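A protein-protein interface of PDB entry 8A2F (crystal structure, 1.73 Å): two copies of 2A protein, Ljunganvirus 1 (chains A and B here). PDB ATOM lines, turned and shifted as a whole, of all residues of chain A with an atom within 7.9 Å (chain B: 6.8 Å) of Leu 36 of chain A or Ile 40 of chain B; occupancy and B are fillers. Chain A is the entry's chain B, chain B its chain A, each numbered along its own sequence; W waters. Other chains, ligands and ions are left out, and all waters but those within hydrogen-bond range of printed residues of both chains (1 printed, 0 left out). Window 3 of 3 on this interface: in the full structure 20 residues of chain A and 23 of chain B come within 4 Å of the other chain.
Leu 36 of chain A touches Leu 36 of chain B (CD2 to CD2, 3.9 Å). Leu 36 of chain A touches Ile 40 of chain B. Leu 122 of chain A touches Leu 36 of chain B (CD1 to CD2, 3.8 Å). Leu 123 of chain A touches His 79 of chain B (O to N, 3.6 Å).
Leu 36 of chain A touches its own counterpart, Leu 36 of chain B. Leu 36 of chain A touches Ile 40 of chain B, but with the chains exchanged Ile 40 of chain A does not touch Leu 36 of chain B (4.2 Å). Of the 5 pairs that touch across the chains among the printed residues, 1 has its exchanged pair printed and touching as well.
The backbone carbonyl oxygen of Leu 122 of chain A lies close to the backbone carbonyl oxygen of Ala 39 of chain B (3.4 Å).
Hydrophobic or aromatic side chains of chain B within 4 Å of the printed part of chain A: Leu 36, Ala 39 and Ile 40. Hydrophobic or aromatic side chains of chain A that line the printed part of chain B: Leu 36 and Leu 122. Among the printed residues, no Asp or Glu carboxylate lies within 4 Å of a Lys or Arg side-chain nitrogen of the other chain.
Of chain B, only Leu 36 and Ile 40 come within 4 Å of Leu 36 of chain A. Ile 40 of chain B touches just one residue of chain A: Leu 36 (3.9 Å). Of the printed residues of chain A, Leu 36 of chain B touches Leu 36 and Leu 122. Printed residues of chain B within 4 Å of Leu 123 of chain A: His 79 (3.6 Å). Of the printed residues of chain A, His 79 of chain B touches Leu 123 (3.6 Å). Of the printed residues of chain B, Leu 122 of chain A touches Leu 36 and Ala 39. The nearest printed residue of chain A that does not touch His 79 of chain B is Val 125 of chain A (4.9 Å).
The backbone NH (N) of Leu 36 of chain A lies within hydrogen-bond range of the side-chain carboxylate (OD1) of Asp 34 of chain A, 2.9 Å away.
Water W1 lies within hydrogen-bond range of ND1 of His 79 of chain B (2.7 Å), O of Ala 39 of chain B (2.7 Å) and O of Leu 122 of chain A (3.5 Å).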
ATOM      1  N   PHE A  15     -22.500 -20.122 -18.728  1.00  0.00           N
ATOM      2  CA  PHE A  15     -22.588 -20.051 -17.276  1.00  0.00           C
ATOM      3  C   PHE A  15     -21.907 -21.265 -16.648  1.00  0.00           C
ATOM      4  O   PHE A  15     -21.860 -21.348 -15.428  1.00  0.00           O
ATOM      5  CB  PHE A  15     -24.025 -19.846 -16.764  1.00  0.00           C
ATOM      6  CG  PHE A  15     -24.993 -20.977 -16.992  1.00  0.00           C
ATOM      7  CD1 PHE A  15     -25.712 -21.056 -18.172  1.00  0.00           C
ATOM      8  CD2 PHE A  15     -25.214 -21.948 -16.023  1.00  0.00           C
ATOM      9  CE1 PHE A  15     -26.601 -22.097 -18.388  1.00  0.00           C
ATOM     10  CE2 PHE A  15     -26.091 -22.997 -16.255  1.00  0.00           C
ATOM     11  CZ  PHE A  15     -26.777 -23.074 -17.443  1.00  0.00           C
ATOM     12  N   TYR A  16     -21.430 -22.205 -17.471  1.00  0.00           N
ATOM     13  CA  TYR A  16     -20.705 -23.368 -16.974  1.00  0.00           C
ATOM     14  C   TYR A  16     -19.863 -23.972 -18.090  1.00  0.00           C
ATOM     15  O   TYR A  16     -19.996 -23.587 -19.251  1.00  0.00           O
ATOM     16  CB  TYR A  16     -21.685 -24.404 -16.418  1.00  0.00           C
ATOM     17  CG  TYR A  16     -22.465 -25.179 -17.449  1.00  0.00           C
ATOM     18  CD1 TYR A  16     -23.560 -24.630 -18.093  1.00  0.00           C
ATOM     19  CD2 TYR A  16     -22.112 -26.479 -17.758  1.00  0.00           C
ATOM     20  CE1 TYR A  16     -24.296 -25.358 -19.013  1.00  0.00           C
ATOM     21  CE2 TYR A  16     -22.837 -27.232 -18.669  1.00  0.00           C
ATOM     22  CZ  TYR A  16     -23.930 -26.659 -19.299  1.00  0.00           C
ATOM     23  OH  TYR A  16     -24.692 -27.353 -20.200  1.00  0.00           O
ATOM     24  N   SER A  32     -26.134 -33.819 -22.844  1.00  0.00           N
ATOM     25  CA  SER A  32     -26.740 -32.991 -21.817  1.00  0.00           C
ATOM     26  C   SER A  32     -27.090 -31.645 -22.446  1.00  0.00           C
ATOM     27  O   SER A  32     -26.234 -31.007 -23.045  1.00  0.00           O
ATOM     28  CB  SER A  32     -25.811 -32.850 -20.630  1.00  0.00           C
ATOM     29  OG  SER A  32     -26.246 -31.813 -19.754  1.00  0.00           O
ATOM     30  N   GLN A  33     -28.359 -31.242 -22.303  1.00  0.00           N
ATOM     31  CA  GLN A  33     -28.813 -29.958 -22.817  1.00  0.00           C
ATOM     32  C   GLN A  33     -28.319 -28.827 -21.913  1.00  0.00           C
ATOM     33  O   GLN A  33     -28.086 -27.723 -22.383  1.00  0.00           O
ATOM     34  CB  GLN A  33     -30.335 -29.956 -22.957  1.00  0.00           C
ATOM     35  CG  GLN A  33     -30.842 -31.022 -23.916  1.00  0.00           C
ATOM     36  CD  GLN A  33     -32.317 -30.876 -24.185  1.00  0.00           C
ATOM     37  OE1 GLN A  33     -33.134 -30.883 -23.266  1.00  0.00           O
ATOM     38  NE2 GLN A  33     -32.666 -30.726 -25.454  1.00  0.00           N
ATOM     39  N   ASP A  34     -28.191 -29.109 -20.615  1.00  0.00           N
ATOM     40  CA  ASP A  34     -27.609 -28.200 -19.649  1.00  0.00           C
ATOM     41  C   ASP A  34     -27.469 -28.928 -18.310  1.00  0.00           C
ATOM     42  O   ASP A  34     -28.242 -29.818 -17.948  1.00  0.00           O
ATOM     43  CB  ASP A  34     -28.371 -26.878 -19.525  1.00  0.00           C
ATOM     44  CG  ASP A  34     -29.617 -26.941 -18.673  1.00  0.00           C
ATOM     45  OD1 ASP A  34     -29.448 -26.987 -17.450  1.00  0.00           O
ATOM     46  OD2 ASP A  34     -30.738 -26.950 -19.237  1.00  0.00           O
ATOM     47  N   ILE A  35     -26.463 -28.492 -17.563  1.00  0.00           N
ATOM     48  CA  ILE A  35     -26.034 -29.172 -16.352  1.00  0.00           C
ATOM     49  C   ILE A  35     -27.131 -29.115 -15.281  1.00  0.00           C
ATOM     50  O   ILE A  35     -27.272 -30.052 -14.505  1.00  0.00           O
ATOM     51  CB  ILE A  35     -24.681 -28.617 -15.863  1.00  0.00           C
ATOM     52  CG1 ILE A  35     -24.131 -29.393 -14.665  1.00  0.00           C
ATOM     53  CG2 ILE A  35     -24.756 -27.126 -15.539  1.00  0.00           C
ATOM     54  CD1 ILE A  35     -23.903 -30.850 -14.915  1.00  0.00           C
ATOM     55  N   LEU A  36     -27.918 -28.033 -15.215  1.00  0.00           N
ATOM     56  CA  LEU A  36     -28.917 -27.896 -14.160  1.00  0.00           C
ATOM     57  C   LEU A  36     -30.004 -28.963 -14.327  1.00  0.00           C
ATOM     58  O   LEU A  36     -30.346 -29.713 -13.397  1.00  0.00           O
ATOM     59  CB  LEU A  36     -29.517 -26.484 -14.230  1.00  0.00           C
ATOM     60  CG  LEU A  36     -28.531 -25.318 -14.316  1.00  0.00           C
ATOM     61  CD1 LEU A  36     -29.267 -24.002 -14.440  1.00  0.00           C
ATOM     62  CD2 LEU A  36     -27.585 -25.274 -13.133  1.00  0.00           C
ATOM     63  N   SER A  37     -30.505 -29.049 -15.560  1.00  0.00           N
ATOM     64  CA  SER A  37     -31.509 -30.024 -15.941  1.00  0.00           C
ATOM     65  C   SER A  37     -30.984 -31.431 -15.654  1.00  0.00           C
ATOM     66  O   SER A  37     -31.661 -32.258 -15.042  1.00  0.00           O
ATOM     67  CB  SER A  37     -31.862 -29.835 -17.391  1.00  0.00           C
ATOM     68  OG  SER A  37     -32.796 -30.803 -17.826  1.00  0.00           O
ATOM     69  N   THR A  38     -29.754 -31.683 -16.092  1.00  0.00           N
ATOM     70  CA  THR A  38     -29.140 -32.994 -15.937  1.00  0.00           C
ATOM     71  C   THR A  38     -29.038 -33.368 -14.459  1.00  0.00           C
ATOM     72  O   THR A  38     -29.380 -34.485 -14.078  1.00  0.00           O
ATOM     73  CB  THR A  38     -27.784 -33.036 -16.640  1.00  0.00           C
ATOM     74  OG1 THR A  38     -28.046 -32.997 -18.046  1.00  0.00           O
ATOM     75  CG2 THR A  38     -26.983 -34.271 -16.303  1.00  0.00           C
ATOM     76  N   ALA A  39     -28.559 -32.437 -13.633  1.00  0.00           N
ATOM     77  CA  ALA A  39     -28.343 -32.690 -12.212  1.00  0.00           C
ATOM     78  C   ALA A  39     -29.638 -33.103 -11.516  1.00  0.00           C
ATOM     79  O   ALA A  39     -29.631 -34.006 -10.679  1.00  0.00           O
ATOM     80  CB  ALA A  39     -27.743 -31.476 -11.540  1.00  0.00           C
ATOM     81  N   ILE A  40     -30.740 -32.422 -11.847  1.00  0.00           N
ATOM     82  CA  ILE A  40     -31.995 -32.670 -11.167  1.00  0.00           C
ATOM     83  C   ILE A  40     -32.620 -33.963 -11.693  1.00  0.00           C
ATOM     84  O   ILE A  40     -33.177 -34.721 -10.906  1.00  0.00           O
ATOM     85  CB  ILE A  40     -32.937 -31.458 -11.330  1.00  0.00           C
ATOM     86  CG1 ILE A  40     -32.351 -30.202 -10.671  1.00  0.00           C
ATOM     87  CG2 ILE A  40     -34.331 -31.788 -10.817  1.00  0.00           C
ATOM     88  CD1 ILE A  40     -31.951 -30.358  -9.231  1.00  0.00           C
ATOM     89  N   THR A  41     -32.525 -34.205 -13.008  1.00  0.00           N
ATOM     90  CA  THR A  41     -33.245 -35.321 -13.615  1.00  0.00           C
ATOM     91  C   THR A  41     -32.603 -36.651 -13.221  1.00  0.00           C
ATOM     92  O   THR A  41     -33.302 -37.666 -13.136  1.00  0.00           O
ATOM     93  CB  THR A  41     -33.316 -35.212 -15.141  1.00  0.00           C
ATOM     94  OG1 THR A  41     -32.003 -35.264 -15.675  1.00  0.00           O
ATOM     95  CG2 THR A  41     -34.010 -33.965 -15.638  1.00  0.00           C
ATOM     96  N   GLY A  42     -31.281 -36.646 -13.033  1.00  0.00           N
ATOM     97  CA  GLY A  42     -30.582 -37.774 -12.441  1.00  0.00           C
ATOM     98  C   GLY A  42     -30.282 -38.890 -13.441  1.00  0.00           C
ATOM     99  O   GLY A  42     -29.985 -39.998 -13.015  1.00  0.00           O
ATOM    100  N   LEU A 115     -19.715 -34.872 -14.452  1.00  0.00           N
ATOM    101  CA  LEU A 115     -20.771 -34.079 -13.840  1.00  0.00           C
ATOM    102  C   LEU A 115     -20.224 -33.222 -12.696  1.00  0.00           C
ATOM    103  O   LEU A 115     -20.651 -32.080 -12.528  1.00  0.00           O
ATOM    104  CB  LEU A 115     -21.882 -34.991 -13.329  1.00  0.00           C
ATOM    105  CG  LEU A 115     -22.792 -35.566 -14.414  1.00  0.00           C
ATOM    106  CD1 LEU A 115     -23.774 -36.573 -13.831  1.00  0.00           C
ATOM    107  CD2 LEU A 115     -23.534 -34.455 -15.160  1.00  0.00           C
ATOM    108  N   SER A 118     -18.302 -30.259 -14.130  1.00  0.00           N
ATOM    109  CA  SER A 118     -19.263 -29.314 -14.692  1.00  0.00           C
ATOM    110  C   SER A 118     -19.990 -28.522 -13.609  1.00  0.00           C
ATOM    111  O   SER A 118     -20.150 -27.312 -13.735  1.00  0.00           O
ATOM    112  CB  SER A 118     -20.251 -30.001 -15.609  1.00  0.00           C
ATOM    113  OG  SER A 118     -19.570 -30.642 -16.685  1.00  0.00           O
ATOM    114  N   LEU A 119     -20.431 -29.184 -12.539  1.00  0.00           N
ATOM    115  CA  LEU A 119     -21.103 -28.496 -11.444  1.00  0.00           C
ATOM    116  C   LEU A 119     -20.177 -27.487 -10.765  1.00  0.00           C
ATOM    117  O   LEU A 119     -20.582 -26.360 -10.473  1.00  0.00           O
ATOM    118  CB  LEU A 119     -21.627 -29.500 -10.416  1.00  0.00           C
ATOM    119  CG  LEU A 119     -22.909 -30.220 -10.812  1.00  0.00           C
ATOM    120  CD1 LEU A 119     -23.189 -31.373  -9.846  1.00  0.00           C
ATOM    121  CD2 LEU A 119     -24.068 -29.267 -10.841  1.00  0.00           C
ATOM    122  N   LEU A 122     -19.568 -23.909 -12.189  1.00  0.00           N
ATOM    123  CA  LEU A 122     -20.511 -22.841 -11.898  1.00  0.00           C
ATOM    124  C   LEU A 122     -19.840 -21.791 -11.009  1.00  0.00           C
ATOM    125  O   LEU A 122     -20.251 -20.644 -11.037  1.00  0.00           O
ATOM    126  CB  LEU A 122     -21.747 -23.415 -11.202  1.00  0.00           C
ATOM    127  CG  LEU A 122     -22.658 -24.314 -12.041  1.00  0.00           C
ATOM    128  CD1 LEU A 122     -23.667 -24.995 -11.121  1.00  0.00           C
ATOM    129  CD2 LEU A 122     -23.382 -23.524 -13.139  1.00  0.00           C
ATOM    130  N   LEU A 123     -18.807 -22.165 -10.217  1.00  0.00           N
ATOM    131  CA  LEU A 123     -18.198 -21.219  -9.281  1.00  0.00           C
ATOM    132  C   LEU A 123     -17.138 -20.340  -9.940  1.00  0.00           C
ATOM    133  O   LEU A 123     -16.739 -19.339  -9.347  1.00  0.00           O
ATOM    134  CB  LEU A 123     -17.563 -21.955  -8.099  1.00  0.00           C
ATOM    135  CG  LEU A 123     -18.496 -22.914  -7.350  1.00  0.00           C
ATOM    136  CD1 LEU A 123     -17.741 -23.633  -6.243  1.00  0.00           C
ATOM    137  CD2 LEU A 123     -19.689 -22.165  -6.794  1.00  0.00           C
ATOM    138  N   VAL A 125     -17.606 -18.652 -12.448  1.00  0.00           N
ATOM    139  CA  VAL A 125     -18.381 -17.517 -12.928  1.00  0.00           C
ATOM    140  C   VAL A 125     -18.468 -17.614 -14.455  1.00  0.00           C
ATOM    141  O   VAL A 125     -19.061 -18.625 -14.894  1.00  0.00           O
ATOM    142  CB  VAL A 125     -17.835 -16.166 -12.419  1.00  0.00           C
ATOM    143  CG1 VAL A 125     -18.296 -14.982 -13.258  1.00  0.00           C
ATOM    144  CG2 VAL A 125     -18.204 -15.954 -10.957  1.00  0.00           C
ATOM    145  N   ILE B  35     -29.005 -24.336  -3.916  1.00  0.00           N
ATOM    146  CA  ILE B  35     -27.567 -24.318  -4.154  1.00  0.00           C
ATOM    147  C   ILE B  35     -27.228 -23.922  -5.593  1.00  0.00           C
ATOM    148  O   ILE B  35     -26.267 -23.190  -5.821  1.00  0.00           O
ATOM    149  CB  ILE B  35     -26.879 -25.623  -3.707  1.00  0.00           C
ATOM    150  CG1 ILE B  35     -25.353 -25.469  -3.728  1.00  0.00           C
ATOM    151  CG2 ILE B  35     -27.340 -26.828  -4.492  1.00  0.00           C
ATOM    152  CD1 ILE B  35     -24.863 -24.358  -2.876  1.00  0.00           C
ATOM    153  N   LEU B  36     -28.013 -24.372  -6.576  1.00  0.00           N
ATOM    154  CA  LEU B  36     -27.703 -24.034  -7.962  1.00  0.00           C
ATOM    155  C   LEU B  36     -27.921 -22.538  -8.194  1.00  0.00           C
ATOM    156  O   LEU B  36     -27.085 -21.908  -8.842  1.00  0.00           O
ATOM    157  CB  LEU B  36     -28.549 -24.908  -8.882  1.00  0.00           C
ATOM    158  CG  LEU B  36     -28.135 -26.379  -8.915  1.00  0.00           C
ATOM    159  CD1 LEU B  36     -29.161 -27.216  -9.678  1.00  0.00           C
ATOM    160  CD2 LEU B  36     -26.767 -26.561  -9.543  1.00  0.00           C
ATOM    161  N   SER B  37     -29.006 -21.985  -7.660  1.00  0.00           N
ATOM    162  CA  SER B  37     -29.235 -20.539  -7.706  1.00  0.00           C
ATOM    163  C   SER B  37     -28.035 -19.771  -7.129  1.00  0.00           C
ATOM    164  O   SER B  37     -27.549 -18.805  -7.722  1.00  0.00           O
ATOM    165  CB  SER B  37     -30.485 -20.182  -6.926  1.00  0.00           C
ATOM    166  OG  SER B  37     -31.623 -20.852  -7.445  1.00  0.00           O
ATOM    167  N   THR B  38     -27.579 -20.215  -5.951  1.00  0.00           N
ATOM    168  CA  THR B  38     -26.462 -19.576  -5.266  1.00  0.00           C
ATOM    169  C   THR B  38     -25.211 -19.600  -6.141  1.00  0.00           C
ATOM    170  O   THR B  38     -24.547 -18.574  -6.311  1.00  0.00           O
ATOM    171  CB  THR B  38     -26.199 -20.222  -3.903  1.00  0.00           C
ATOM    172  OG1 THR B  38     -27.312 -19.903  -3.075  1.00  0.00           O
ATOM    173  CG2 THR B  38     -24.908 -19.732  -3.270  1.00  0.00           C
ATOM    174  N   ALA B  39     -24.888 -20.771  -6.710  1.00  0.00           N
ATOM    175  CA  ALA B  39     -23.716 -20.906  -7.570  1.00  0.00           C
ATOM    176  C   ALA B  39     -23.769 -19.983  -8.800  1.00  0.00           C
ATOM    177  O   ALA B  39     -22.769 -19.387  -9.166  1.00  0.00           O
ATOM    178  CB  ALA B  39     -23.589 -22.336  -7.970  1.00  0.00           C
ATOM    179  N   ILE B  40     -24.940 -19.822  -9.406  1.00  0.00           N
ATOM    180  CA  ILE B  40     -25.094 -18.964 -10.571  1.00  0.00           C
ATOM    181  C   ILE B  40     -24.947 -17.492 -10.194  1.00  0.00           C
ATOM    182  O   ILE B  40     -24.368 -16.718 -10.957  1.00  0.00           O
ATOM    183  CB  ILE B  40     -26.427 -19.267 -11.284  1.00  0.00           C
ATOM    184  CG1 ILE B  40     -26.354 -20.639 -11.958  1.00  0.00           C
ATOM    185  CG2 ILE B  40     -26.781 -18.183 -12.291  1.00  0.00           C
ATOM    186  CD1 ILE B  40     -27.679 -21.263 -12.230  1.00  0.00           C
ATOM    187  N   THR B  41     -25.473 -17.107  -9.026  1.00  0.00           N
ATOM    188  CA  THR B  41     -25.454 -15.715  -8.591  1.00  0.00           C
ATOM    189  C   THR B  41     -24.023 -15.232  -8.358  1.00  0.00           C
ATOM    190  O   THR B  41     -23.698 -14.062  -8.607  1.00  0.00           O
ATOM    191  CB  THR B  41     -26.305 -15.520  -7.332  1.00  0.00           C
ATOM    192  OG1 THR B  41     -27.661 -15.883  -7.621  1.00  0.00           O
ATOM    193  CG2 THR B  41     -26.240 -14.102  -6.806  1.00  0.00           C
ATOM    194  N   GLY B  42     -23.209 -16.131  -7.786  1.00  0.00           N
ATOM    195  CA  GLY B  42     -21.782 -15.922  -7.608  1.00  0.00           C
ATOM    196  C   GLY B  42     -21.433 -15.100  -6.370  1.00  0.00           C
ATOM    197  O   GLY B  42     -20.284 -14.691  -6.181  1.00  0.00           O
ATOM    198  N   LYS B  43     -22.429 -14.851  -5.516  1.00  0.00           N
ATOM    199  CA  LYS B  43     -22.222 -14.169  -4.248  1.00  0.00           C
ATOM    200  C   LYS B  43     -23.139 -14.778  -3.199  1.00  0.00           C
ATOM    201  O   LYS B  43     -24.241 -15.217  -3.538  1.00  0.00           O
ATOM    202  CB  LYS B  43     -22.545 -12.677  -4.346  1.00  0.00           C
ATOM    203  CG  LYS B  43     -21.828 -11.908  -5.436  1.00  0.00           C
ATOM    204  CD  LYS B  43     -22.270 -10.459  -5.499  1.00  0.00           C
ATOM    205  CE  LYS B  43     -21.577  -9.699  -6.611  1.00  0.00           C
ATOM    206  NZ  LYS B  43     -21.851  -8.245  -6.530  1.00  0.00           N
ATOM    207  N   HIS B  79     -16.460 -17.048  -6.554  1.00  0.00           N
ATOM    208  CA  HIS B  79     -17.583 -16.692  -5.698  1.00  0.00           C
ATOM    209  C   HIS B  79     -17.166 -15.696  -4.615  1.00  0.00           C
ATOM    210  O   HIS B  79     -16.080 -15.830  -4.045  1.00  0.00           O
ATOM    211  CB  HIS B  79     -18.140 -17.963  -5.100  1.00  0.00           C
ATOM    212  CG  HIS B  79     -19.544 -17.845  -4.616  1.00  0.00           C
ATOM    213  ND1 HIS B  79     -20.598 -18.276  -5.378  1.00  0.00           N
ATOM    214  CD2 HIS B  79     -20.074 -17.424  -3.433  1.00  0.00           C
ATOM    215  CE1 HIS B  79     -21.714 -18.103  -4.692  1.00  0.00           C
ATOM    216  NE2 HIS B  79     -21.426 -17.593  -3.512  1.00  0.00           N
HETATM  217  O   HOH W   1     -20.331 -19.109  -7.935  1.00  0.00           O
